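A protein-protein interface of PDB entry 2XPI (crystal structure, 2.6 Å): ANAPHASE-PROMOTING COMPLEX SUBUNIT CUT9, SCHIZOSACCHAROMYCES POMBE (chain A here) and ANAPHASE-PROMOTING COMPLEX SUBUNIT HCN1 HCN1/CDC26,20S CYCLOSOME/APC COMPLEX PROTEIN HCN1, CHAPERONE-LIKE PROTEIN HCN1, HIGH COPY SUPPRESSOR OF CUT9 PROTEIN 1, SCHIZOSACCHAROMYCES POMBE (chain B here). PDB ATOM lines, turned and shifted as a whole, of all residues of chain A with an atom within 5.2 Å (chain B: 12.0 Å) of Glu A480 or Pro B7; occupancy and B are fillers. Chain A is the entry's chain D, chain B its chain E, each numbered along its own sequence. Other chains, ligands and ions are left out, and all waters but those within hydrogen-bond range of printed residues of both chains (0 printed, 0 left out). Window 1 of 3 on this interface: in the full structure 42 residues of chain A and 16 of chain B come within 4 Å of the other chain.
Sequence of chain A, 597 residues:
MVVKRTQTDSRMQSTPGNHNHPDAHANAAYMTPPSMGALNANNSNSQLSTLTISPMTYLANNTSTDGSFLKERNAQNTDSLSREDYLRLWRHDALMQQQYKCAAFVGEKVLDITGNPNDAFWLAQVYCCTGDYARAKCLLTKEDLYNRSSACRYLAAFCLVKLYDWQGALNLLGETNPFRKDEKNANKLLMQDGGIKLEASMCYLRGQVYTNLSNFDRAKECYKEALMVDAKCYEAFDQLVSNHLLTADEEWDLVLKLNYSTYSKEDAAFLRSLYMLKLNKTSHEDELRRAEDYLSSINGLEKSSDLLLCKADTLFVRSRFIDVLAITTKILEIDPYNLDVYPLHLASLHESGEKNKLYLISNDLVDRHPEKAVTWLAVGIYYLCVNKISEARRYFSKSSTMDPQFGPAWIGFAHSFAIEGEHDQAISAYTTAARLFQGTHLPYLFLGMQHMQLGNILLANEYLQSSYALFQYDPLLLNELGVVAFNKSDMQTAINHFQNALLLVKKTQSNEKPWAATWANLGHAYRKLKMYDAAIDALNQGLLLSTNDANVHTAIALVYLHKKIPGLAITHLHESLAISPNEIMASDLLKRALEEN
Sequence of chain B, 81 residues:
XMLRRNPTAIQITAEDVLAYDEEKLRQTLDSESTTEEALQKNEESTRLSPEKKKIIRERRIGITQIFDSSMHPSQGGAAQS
The backbone carbonyl oxygen (O) of Thr B8 sits at hydrogen-bond distance from the side-chain amide nitrogen (ND2) of Asn A479, at 3.1 Å. OE1 of Glu A480 is in hydrogen-bond range of OG1 of Thr B8 (2.5 Å).
The backbone carbonyl oxygen (O) of Met A449 sits close to the side-chain amide oxygen (OE1) of Gln A453, 2.7 Å away. The side-chain hydroxyl (OG1) of Thr A518 sits at hydrogen-bond distance from the side-chain amide oxygen (OD1) of Asn A479 (3.2 Å). The side-chain amide nitrogen of Asn A479 sits at hydrogen-bond distance from the side-chain carboxylate of Glu A480 (3.0 Å).
Among the printed residues, pairs that only touch across the chains: Met A449 with Asn B6 (3.2 Å), Met A449 with Thr B8 (3.9 Å), Gln A453 with Thr B8 (3.4 Å), Leu A476 with Arg B4 (3.7 Å), Leu A476 with Arg B5 (3.7 Å), Leu A476 with Pro B7 (3.7 Å), Asn A479 with Pro B7 (3.7 Å), Glu A480 with Pro B7 (3.7 Å), Val A483 with Ile B10 (3.9 Å), Pro A514 with Asn B6 (3.5 Å), Pro A514 with Pro B7 (3.8 Å), Trp A515 with Pro B7 (3.4 Å), Ala A517 with Pro B7 (3.7 Å), Ala A517 with Thr B8 (3.9 Å), Ala A517 with Ala B9 (3.8 Å) and Thr A518 with Pro B7 (3.96 Å).
Of the printed residues of chain B, Glu A480 touches Pro B7 and Thr B8. No residue of chain B comes within 4 Å of Leu A464. Leu A476 touches three residues of chain B. No residue of chain B comes within 4 Å of Leu A477. Of chain B, only Pro B7 (3.7 Å) and Thr B8 (3.1 Å) come within 4 Å of Asn A479. Val A483 touches one residue of chain B. No residue of chain B comes within 4 Å of Val A484. Of chain B, only Asn B6 and Pro B7 come within 4 Å of Pro A514. Trp A515 touches just one residue of chain B: Pro B7 (3.4 Å). Printed residues of chain B within 4 Å of Ala A517: Pro B7 (3.7 Å), Thr B8 (3.9 Å) and Ala B9 (3.8 Å). Printed residues of chain A within 4 Å of Asn B6: Met A449 and Pro A514. Of the printed residues of chain A, Thr B8 touches Met A449, Gln A453, Asn A479, Glu A480 and Ala A517. Leu A478 touches none of the printed residues of chain B. Gln B11 touches none of the printed residues of chain A. The nearest residue of chain B that does not touch Glu A480 is Asn B6 (4.6 Å). The nearest residue of chain A that does not touch Pro B7 is Met A449 (4.7 Å).
Printed residues of chain A that touch a printed residue of chain B: Met A449, Gln A453, Leu A476, Asn A479, Glu A480, Val A483, Pro A514, Trp A515, Ala A517 and Thr A518. Of the 9 printed residues of chain B, 7 touch a printed residue of chain A. Hydrophobic or aromatic side chains of chain B within 4 Å of the printed part of chain A: Pro B7, Ala B9 and Ile B10.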
ATOM      1  N   LEU A 445     -15.207 -24.252  14.561  1.00  0.00           N
ATOM      2  CA  LEU A 445     -15.800 -23.126  15.220  1.00  0.00           C
ATOM      3  C   LEU A 445     -15.566 -21.857  14.388  1.00  0.00           C
ATOM      4  O   LEU A 445     -16.517 -21.154  14.051  1.00  0.00           O
ATOM      5  CB  LEU A 445     -15.189 -23.006  16.600  1.00  0.00           C
ATOM      6  CG  LEU A 445     -15.944 -22.254  17.685  1.00  0.00           C
ATOM      7  CD1 LEU A 445     -14.910 -21.610  18.585  1.00  0.00           C
ATOM      8  CD2 LEU A 445     -16.856 -21.203  17.110  1.00  0.00           C
ATOM      9  N   MET A 449     -18.135 -19.284  12.648  1.00  0.00           N
ATOM     10  CA  MET A 449     -18.233 -17.847  12.906  1.00  0.00           C
ATOM     11  C   MET A 449     -18.180 -17.042  11.618  1.00  0.00           C
ATOM     12  O   MET A 449     -18.836 -16.006  11.507  1.00  0.00           O
ATOM     13  CB  MET A 449     -17.123 -17.379  13.848  1.00  0.00           C
ATOM     14  CG  MET A 449     -17.252 -17.947  15.250  1.00  0.00           C
ATOM     15  SD  MET A 449     -15.862 -17.509  16.299  1.00  0.00           S
ATOM     16  CE  MET A 449     -16.233 -15.798  16.665  1.00  0.00           C
ATOM     17  N   MET A 452     -21.415 -17.181   9.626  1.00  0.00           N
ATOM     18  CA  MET A 452     -22.463 -16.439  10.297  1.00  0.00           C
ATOM     19  C   MET A 452     -22.355 -14.966   9.933  1.00  0.00           C
ATOM     20  O   MET A 452     -23.365 -14.328   9.652  1.00  0.00           O
ATOM     21  CB  MET A 452     -22.447 -16.653  11.804  1.00  0.00           C
ATOM     22  CG  MET A 452     -23.803 -17.064  12.341  1.00  0.00           C
ATOM     23  SD  MET A 452     -23.791 -17.070  14.136  1.00  0.00           S
ATOM     24  CE  MET A 452     -22.202 -17.844  14.439  1.00  0.00           C
ATOM     25  N   GLN A 453     -21.132 -14.441   9.898  1.00  0.00           N
ATOM     26  CA  GLN A 453     -20.900 -13.067   9.449  1.00  0.00           C
ATOM     27  C   GLN A 453     -21.352 -12.867   8.002  1.00  0.00           C
ATOM     28  O   GLN A 453     -21.878 -11.822   7.642  1.00  0.00           O
ATOM     29  CB  GLN A 453     -19.433 -12.687   9.616  1.00  0.00           C
ATOM     30  CG  GLN A 453     -19.101 -12.029  10.953  1.00  0.00           C
ATOM     31  CD  GLN A 453     -19.935 -12.564  12.133  1.00  0.00           C
ATOM     32  OE1 GLN A 453     -19.856 -13.749  12.499  1.00  0.00           O
ATOM     33  NE2 GLN A 453     -20.724 -11.672  12.750  1.00  0.00           N
ATOM     34  N   LEU A 464     -20.705 -25.331  13.416  1.00  0.00           N
ATOM     35  CA  LEU A 464     -20.801 -25.215  14.868  1.00  0.00           C
ATOM     36  C   LEU A 464     -21.195 -26.544  15.494  1.00  0.00           C
ATOM     37  O   LEU A 464     -20.634 -26.938  16.506  1.00  0.00           O
ATOM     38  CB  LEU A 464     -21.789 -24.123  15.258  1.00  0.00           C
ATOM     39  CG  LEU A 464     -21.295 -22.753  14.800  1.00  0.00           C
ATOM     40  CD1 LEU A 464     -22.236 -21.650  15.236  1.00  0.00           C
ATOM     41  CD2 LEU A 464     -19.900 -22.522  15.343  1.00  0.00           C
ATOM     42  N   LEU A 476     -16.861 -19.812  23.832  1.00  0.00           N
ATOM     43  CA  LEU A 476     -16.921 -19.116  22.550  1.00  0.00           C
ATOM     44  C   LEU A 476     -17.859 -19.877  21.615  1.00  0.00           C
ATOM     45  O   LEU A 476     -18.607 -19.287  20.838  1.00  0.00           O
ATOM     46  CB  LEU A 476     -15.526 -19.029  21.931  1.00  0.00           C
ATOM     47  CG  LEU A 476     -15.173 -17.956  20.886  1.00  0.00           C
ATOM     48  CD1 LEU A 476     -14.363 -18.572  19.736  1.00  0.00           C
ATOM     49  CD2 LEU A 476     -16.376 -17.190  20.354  1.00  0.00           C
ATOM     50  N   LEU A 477     -17.822 -21.198  21.696  1.00  0.00           N
ATOM     51  CA  LEU A 477     -18.656 -22.011  20.832  1.00  0.00           C
ATOM     52  C   LEU A 477     -20.114 -21.893  21.239  1.00  0.00           C
ATOM     53  O   LEU A 477     -20.998 -21.853  20.383  1.00  0.00           O
ATOM     54  CB  LEU A 477     -18.198 -23.461  20.889  1.00  0.00           C
ATOM     55  CG  LEU A 477     -19.201 -24.538  20.525  1.00  0.00           C
ATOM     56  CD1 LEU A 477     -19.532 -24.518  19.059  1.00  0.00           C
ATOM     57  CD2 LEU A 477     -18.641 -25.885  20.934  1.00  0.00           C
ATOM     58  N   LEU A 478     -20.352 -21.842  22.553  1.00  0.00           N
ATOM     59  CA  LEU A 478     -21.692 -21.672  23.097  1.00  0.00           C
ATOM     60  C   LEU A 478     -22.263 -20.308  22.752  1.00  0.00           C
ATOM     61  O   LEU A 478     -23.463 -20.175  22.512  1.00  0.00           O
ATOM     62  CB  LEU A 478     -21.706 -21.885  24.611  1.00  0.00           C
ATOM     63  CG  LEU A 478     -21.379 -23.318  25.021  1.00  0.00           C
ATOM     64  CD1 LEU A 478     -21.736 -23.505  26.455  1.00  0.00           C
ATOM     65  CD2 LEU A 478     -22.164 -24.281  24.175  1.00  0.00           C
ATOM     66  N   ASN A 479     -21.414 -19.286  22.714  1.00  0.00           N
ATOM     67  CA  ASN A 479     -21.895 -18.012  22.211  1.00  0.00           C
ATOM     68  C   ASN A 479     -22.367 -18.123  20.761  1.00  0.00           C
ATOM     69  O   ASN A 479     -23.431 -17.607  20.421  1.00  0.00           O
ATOM     70  CB  ASN A 479     -20.879 -16.902  22.359  1.00  0.00           C
ATOM     71  CG  ASN A 479     -21.422 -15.567  21.891  1.00  0.00           C
ATOM     72  OD1 ASN A 479     -22.110 -14.874  22.642  1.00  0.00           O
ATOM     73  ND2 ASN A 479     -21.133 -15.203  20.642  1.00  0.00           N
ATOM     74  N   GLU A 480     -21.608 -18.812  19.909  1.00  0.00           N
ATOM     75  CA  GLU A 480     -21.994 -18.878  18.508  1.00  0.00           C
ATOM     76  C   GLU A 480     -23.264 -19.707  18.289  1.00  0.00           C
ATOM     77  O   GLU A 480     -24.106 -19.328  17.495  1.00  0.00           O
ATOM     78  CB  GLU A 480     -20.844 -19.358  17.630  1.00  0.00           C
ATOM     79  CG  GLU A 480     -19.558 -18.561  17.825  1.00  0.00           C
ATOM     80  CD  GLU A 480     -19.762 -17.044  17.688  1.00  0.00           C
ATOM     81  OE1 GLU A 480     -20.429 -16.617  16.716  1.00  0.00           O
ATOM     82  OE2 GLU A 480     -19.255 -16.287  18.554  1.00  0.00           O
ATOM     83  N   LEU A 481     -23.408 -20.830  18.983  1.00  0.00           N
ATOM     84  CA  LEU A 481     -24.658 -21.580  18.917  1.00  0.00           C
ATOM     85  C   LEU A 481     -25.813 -20.690  19.347  1.00  0.00           C
ATOM     86  O   LEU A 481     -26.907 -20.735  18.771  1.00  0.00           O
ATOM     87  CB  LEU A 481     -24.603 -22.825  19.802  1.00  0.00           C
ATOM     88  CG  LEU A 481     -23.693 -23.927  19.262  1.00  0.00           C
ATOM     89  CD1 LEU A 481     -23.527 -25.043  20.269  1.00  0.00           C
ATOM     90  CD2 LEU A 481     -24.253 -24.451  17.952  1.00  0.00           C
ATOM     91  N   GLY A 482     -25.567 -19.873  20.357  1.00  0.00           N
ATOM     92  CA  GLY A 482     -26.606 -19.004  20.857  1.00  0.00           C
ATOM     93  C   GLY A 482     -27.056 -18.053  19.771  1.00  0.00           C
ATOM     94  O   GLY A 482     -28.252 -17.812  19.610  1.00  0.00           O
ATOM     95  N   VAL A 483     -26.095 -17.523  19.015  1.00  0.00           N
ATOM     96  CA  VAL A 483     -26.380 -16.500  18.021  1.00  0.00           C
ATOM     97  C   VAL A 483     -27.059 -17.113  16.812  1.00  0.00           C
ATOM     98  O   VAL A 483     -27.825 -16.451  16.121  1.00  0.00           O
ATOM     99  CB  VAL A 483     -25.102 -15.728  17.605  1.00  0.00           C
ATOM    100  CG1 VAL A 483     -25.352 -14.867  16.361  1.00  0.00           C
ATOM    101  CG2 VAL A 483     -24.625 -14.884  18.741  1.00  0.00           C
ATOM    102  N   VAL A 484     -26.785 -18.387  16.559  1.00  0.00           N
ATOM    103  CA  VAL A 484     -27.501 -19.102  15.515  1.00  0.00           C
ATOM    104  C   VAL A 484     -28.934 -19.356  15.978  1.00  0.00           C
ATOM    105  O   VAL A 484     -29.886 -19.118  15.228  1.00  0.00           O
ATOM    106  CB  VAL A 484     -26.841 -20.440  15.165  1.00  0.00           C
ATOM    107  CG1 VAL A 484     -27.635 -21.131  14.085  1.00  0.00           C
ATOM    108  CG2 VAL A 484     -25.421 -20.233  14.715  1.00  0.00           C
ATOM    109  N   ALA A 485     -29.095 -19.837  17.210  1.00  0.00           N
ATOM    110  CA  ALA A 485     -30.442 -20.095  17.712  1.00  0.00           C
ATOM    111  C   ALA A 485     -31.203 -18.805  17.623  1.00  0.00           C
ATOM    112  O   ALA A 485     -32.364 -18.787  17.240  1.00  0.00           O
ATOM    113  CB  ALA A 485     -30.431 -20.599  19.131  1.00  0.00           C
ATOM    114  N   PRO A 514     -14.074  -9.022  26.090  1.00  0.00           N
ATOM    115  CA  PRO A 514     -14.740  -9.526  24.879  1.00  0.00           C
ATOM    116  C   PRO A 514     -16.100 -10.146  25.182  1.00  0.00           C
ATOM    117  O   PRO A 514     -16.987 -10.094  24.320  1.00  0.00           O
ATOM    118  CB  PRO A 514     -13.755 -10.575  24.335  1.00  0.00           C
ATOM    119  CG  PRO A 514     -12.436 -10.253  25.009  1.00  0.00           C
ATOM    120  CD  PRO A 514     -12.794  -9.712  26.353  1.00  0.00           C
ATOM    121  N   TRP A 515     -16.260 -10.705  26.383  1.00  0.00           N
ATOM    122  CA  TRP A 515     -17.514 -11.339  26.794  1.00  0.00           C
ATOM    123  C   TRP A 515     -18.668 -10.375  27.044  1.00  0.00           C
ATOM    124  O   TRP A 515     -19.807 -10.791  27.229  1.00  0.00           O
ATOM    125  CB  TRP A 515     -17.276 -12.234  27.997  1.00  0.00           C
ATOM    126  CG  TRP A 515     -16.286 -13.257  27.642  1.00  0.00           C
ATOM    127  CD1 TRP A 515     -14.997 -13.295  28.023  1.00  0.00           C
ATOM    128  CD2 TRP A 515     -16.485 -14.378  26.766  1.00  0.00           C
ATOM    129  NE1 TRP A 515     -14.371 -14.383  27.467  1.00  0.00           N
ATOM    130  CE2 TRP A 515     -15.259 -15.058  26.682  1.00  0.00           C
ATOM    131  CE3 TRP A 515     -17.584 -14.877  26.061  1.00  0.00           C
ATOM    132  CZ2 TRP A 515     -15.088 -16.207  25.914  1.00  0.00           C
ATOM    133  CZ3 TRP A 515     -17.420 -16.024  25.307  1.00  0.00           C
ATOM    134  CH2 TRP A 515     -16.177 -16.677  25.238  1.00  0.00           C
ATOM    135  N   ALA A 517     -19.902  -9.023  24.783  1.00  0.00           N
ATOM    136  CA  ALA A 517     -20.787  -9.380  23.670  1.00  0.00           C
ATOM    137  C   ALA A 517     -21.790 -10.455  24.048  1.00  0.00           C
ATOM    138  O   ALA A 517     -22.897 -10.482  23.517  1.00  0.00           O
ATOM    139  CB  ALA A 517     -20.006  -9.807  22.417  1.00  0.00           C
ATOM    140  N   THR A 518     -21.403 -11.353  24.947  1.00  0.00           N
ATOM    141  CA  THR A 518     -22.298 -12.433  25.365  1.00  0.00           C
ATOM    142  C   THR A 518     -23.359 -11.883  26.305  1.00  0.00           C
ATOM    143  O   THR A 518     -24.512 -12.265  26.229  1.00  0.00           O
ATOM    144  CB  THR A 518     -21.547 -13.583  26.047  1.00  0.00           C
ATOM    145  OG1 THR A 518     -20.434 -13.958  25.240  1.00  0.00           O
ATOM    146  CG2 THR A 518     -22.436 -14.779  26.197  1.00  0.00           C
ATOM    147  N   LEU B   3      -4.585 -19.369  18.078  1.00  0.00           N
ATOM    148  CA  LEU B   3      -5.187 -18.066  18.262  1.00  0.00           C
ATOM    149  C   LEU B   3      -6.704 -18.172  18.265  1.00  0.00           C
ATOM    150  O   LEU B   3      -7.297 -18.782  17.380  1.00  0.00           O
ATOM    151  CB  LEU B   3      -4.785 -17.134  17.126  1.00  0.00           C
ATOM    152  CG  LEU B   3      -3.553 -16.255  17.314  1.00  0.00           C
ATOM    153  CD1 LEU B   3      -2.601 -16.890  18.310  1.00  0.00           C
ATOM    154  CD2 LEU B   3      -2.862 -15.992  15.979  1.00  0.00           C
ATOM    155  N   ARG B   4      -7.333 -17.542  19.246  1.00  0.00           N
ATOM    156  CA  ARG B   4      -8.777 -17.490  19.299  1.00  0.00           C
ATOM    157  C   ARG B   4      -9.259 -16.175  18.733  1.00  0.00           C
ATOM    158  O   ARG B   4      -8.472 -15.337  18.332  1.00  0.00           O
ATOM    159  CB  ARG B   4      -9.252 -17.622  20.745  1.00  0.00           C
ATOM    160  CG  ARG B   4      -8.691 -18.815  21.451  1.00  0.00           C
ATOM    161  CD  ARG B   4      -9.205 -18.858  22.861  1.00  0.00           C
ATOM    162  NE  ARG B   4      -9.812 -20.158  23.091  1.00  0.00           N
ATOM    163  CZ  ARG B   4     -11.113 -20.410  23.015  1.00  0.00           C
ATOM    164  NH1 ARG B   4     -11.973 -19.439  22.771  1.00  0.00           N
ATOM    165  NH2 ARG B   4     -11.543 -21.641  23.211  1.00  0.00           N
ATOM    166  N   ARG B   5     -10.565 -15.998  18.691  1.00  0.00           N
ATOM    167  CA  ARG B   5     -11.121 -14.692  18.414  1.00  0.00           C
ATOM    168  C   ARG B   5     -12.312 -14.420  19.312  1.00  0.00           C
ATOM    169  O   ARG B   5     -12.671 -15.253  20.147  1.00  0.00           O
ATOM    170  CB  ARG B   5     -11.498 -14.552  16.948  1.00  0.00           C
ATOM    171  CG  ARG B   5     -12.132 -15.759  16.357  1.00  0.00           C
ATOM    172  CD  ARG B   5     -12.109 -15.637  14.848  1.00  0.00           C
ATOM    173  NE  ARG B   5     -13.054 -14.648  14.345  1.00  0.00           N
ATOM    174  CZ  ARG B   5     -13.735 -14.803  13.215  1.00  0.00           C
ATOM    175  NH1 ARG B   5     -13.567 -15.910  12.484  1.00  0.00           N
ATOM    176  NH2 ARG B   5     -14.578 -13.860  12.809  1.00  0.00           N
ATOM    177  N   ASN B   6     -12.919 -13.253  19.136  1.00  0.00           N
ATOM    178  CA  ASN B   6     -13.952 -12.778  20.055  1.00  0.00           C
ATOM    179  C   ASN B   6     -15.390 -13.163  19.716  1.00  0.00           C
ATOM    180  O   ASN B   6     -15.766 -13.257  18.540  1.00  0.00           O
ATOM    181  CB  ASN B   6     -13.846 -11.263  20.212  1.00  0.00           C
ATOM    182  CG  ASN B   6     -12.571 -10.840  20.933  1.00  0.00           C
ATOM    183  OD1 ASN B   6     -12.158  -9.685  20.836  1.00  0.00           O
ATOM    184  ND2 ASN B   6     -11.936 -11.781  21.645  1.00  0.00           N
ATOM    185  N   PRO B   7     -16.204 -13.377  20.765  1.00  0.00           N
ATOM    186  CA  PRO B   7     -17.630 -13.675  20.619  1.00  0.00           C
ATOM    187  C   PRO B   7     -18.291 -12.730  19.624  1.00  0.00           C
ATOM    188  O   PRO B   7     -18.113 -11.525  19.712  1.00  0.00           O
ATOM    189  CB  PRO B   7     -18.186 -13.427  22.029  1.00  0.00           C
ATOM    190  CG  PRO B   7     -17.033 -13.642  22.948  1.00  0.00           C
ATOM    191  CD  PRO B   7     -15.802 -13.248  22.180  1.00  0.00           C
ATOM    192  N   THR B   8     -19.017 -13.290  18.665  1.00  0.00           N
ATOM    193  CA  THR B   8     -19.920 -12.527  17.812  1.00  0.00           C
ATOM    194  C   THR B   8     -20.941 -11.759  18.666  1.00  0.00           C
ATOM    195  O   THR B   8     -21.387 -12.221  19.721  1.00  0.00           O
ATOM    196  CB  THR B   8     -20.714 -13.469  16.862  1.00  0.00           C
ATOM    197  OG1 THR B   8     -19.812 -14.267  16.094  1.00  0.00           O
ATOM    198  CG2 THR B   8     -21.591 -12.671  15.921  1.00  0.00           C
ATOM    199  N   ALA B   9     -21.346 -10.602  18.177  1.00  0.00           N
ATOM    200  CA  ALA B   9     -22.295  -9.796  18.900  1.00  0.00           C
ATOM    201  C   ALA B   9     -23.542  -9.574  18.064  1.00  0.00           C
ATOM    202  O   ALA B   9     -23.479  -9.006  16.988  1.00  0.00           O
ATOM    203  CB  ALA B   9     -21.664  -8.470  19.262  1.00  0.00           C
ATOM    204  N   ILE B  10     -24.687 -10.022  18.559  1.00  0.00           N
ATOM    205  CA  ILE B  10     -25.936  -9.606  17.954  1.00  0.00           C
ATOM    206  C   ILE B  10     -26.003  -8.073  18.046  1.00  0.00           C
ATOM    207  O   ILE B  10     -25.620  -7.493  19.070  1.00  0.00           O
ATOM    208  CB  ILE B  10     -27.119 -10.230  18.684  1.00  0.00           C
ATOM    209  CG1 ILE B  10     -27.019 -11.752  18.645  1.00  0.00           C
ATOM    210  CG2 ILE B  10     -28.431  -9.763  18.078  1.00  0.00           C
ATOM    211  CD1 ILE B  10     -27.729 -12.418  19.814  1.00  0.00           C
ATOM    212  N   GLN B  11     -26.465  -7.426  16.975  1.00  0.00           N
ATOM    213  CA  GLN B  11     -26.591  -5.968  16.928  1.00  0.00           C
ATOM    214  C   GLN B  11     -28.043  -5.559  16.765  1.00  0.00           C
ATOM    215  O   GLN B  11     -28.887  -6.385  16.442  1.00  0.00           O
ATOM    216  CB  GLN B  11     -25.796  -5.414  15.755  1.00  0.00           C
ATOM    217  CG  GLN B  11     -24.306  -5.628  15.873  1.00  0.00           C
ATOM    218  CD  GLN B  11     -23.671  -4.663  16.851  1.00  0.00           C
ATOM    219  OE1 GLN B  11     -23.475  -4.981  18.027  1.00  0.00           O
ATOM    220  NE2 GLN B  11     -23.353  -3.467  16.370  1.00  0.00           N
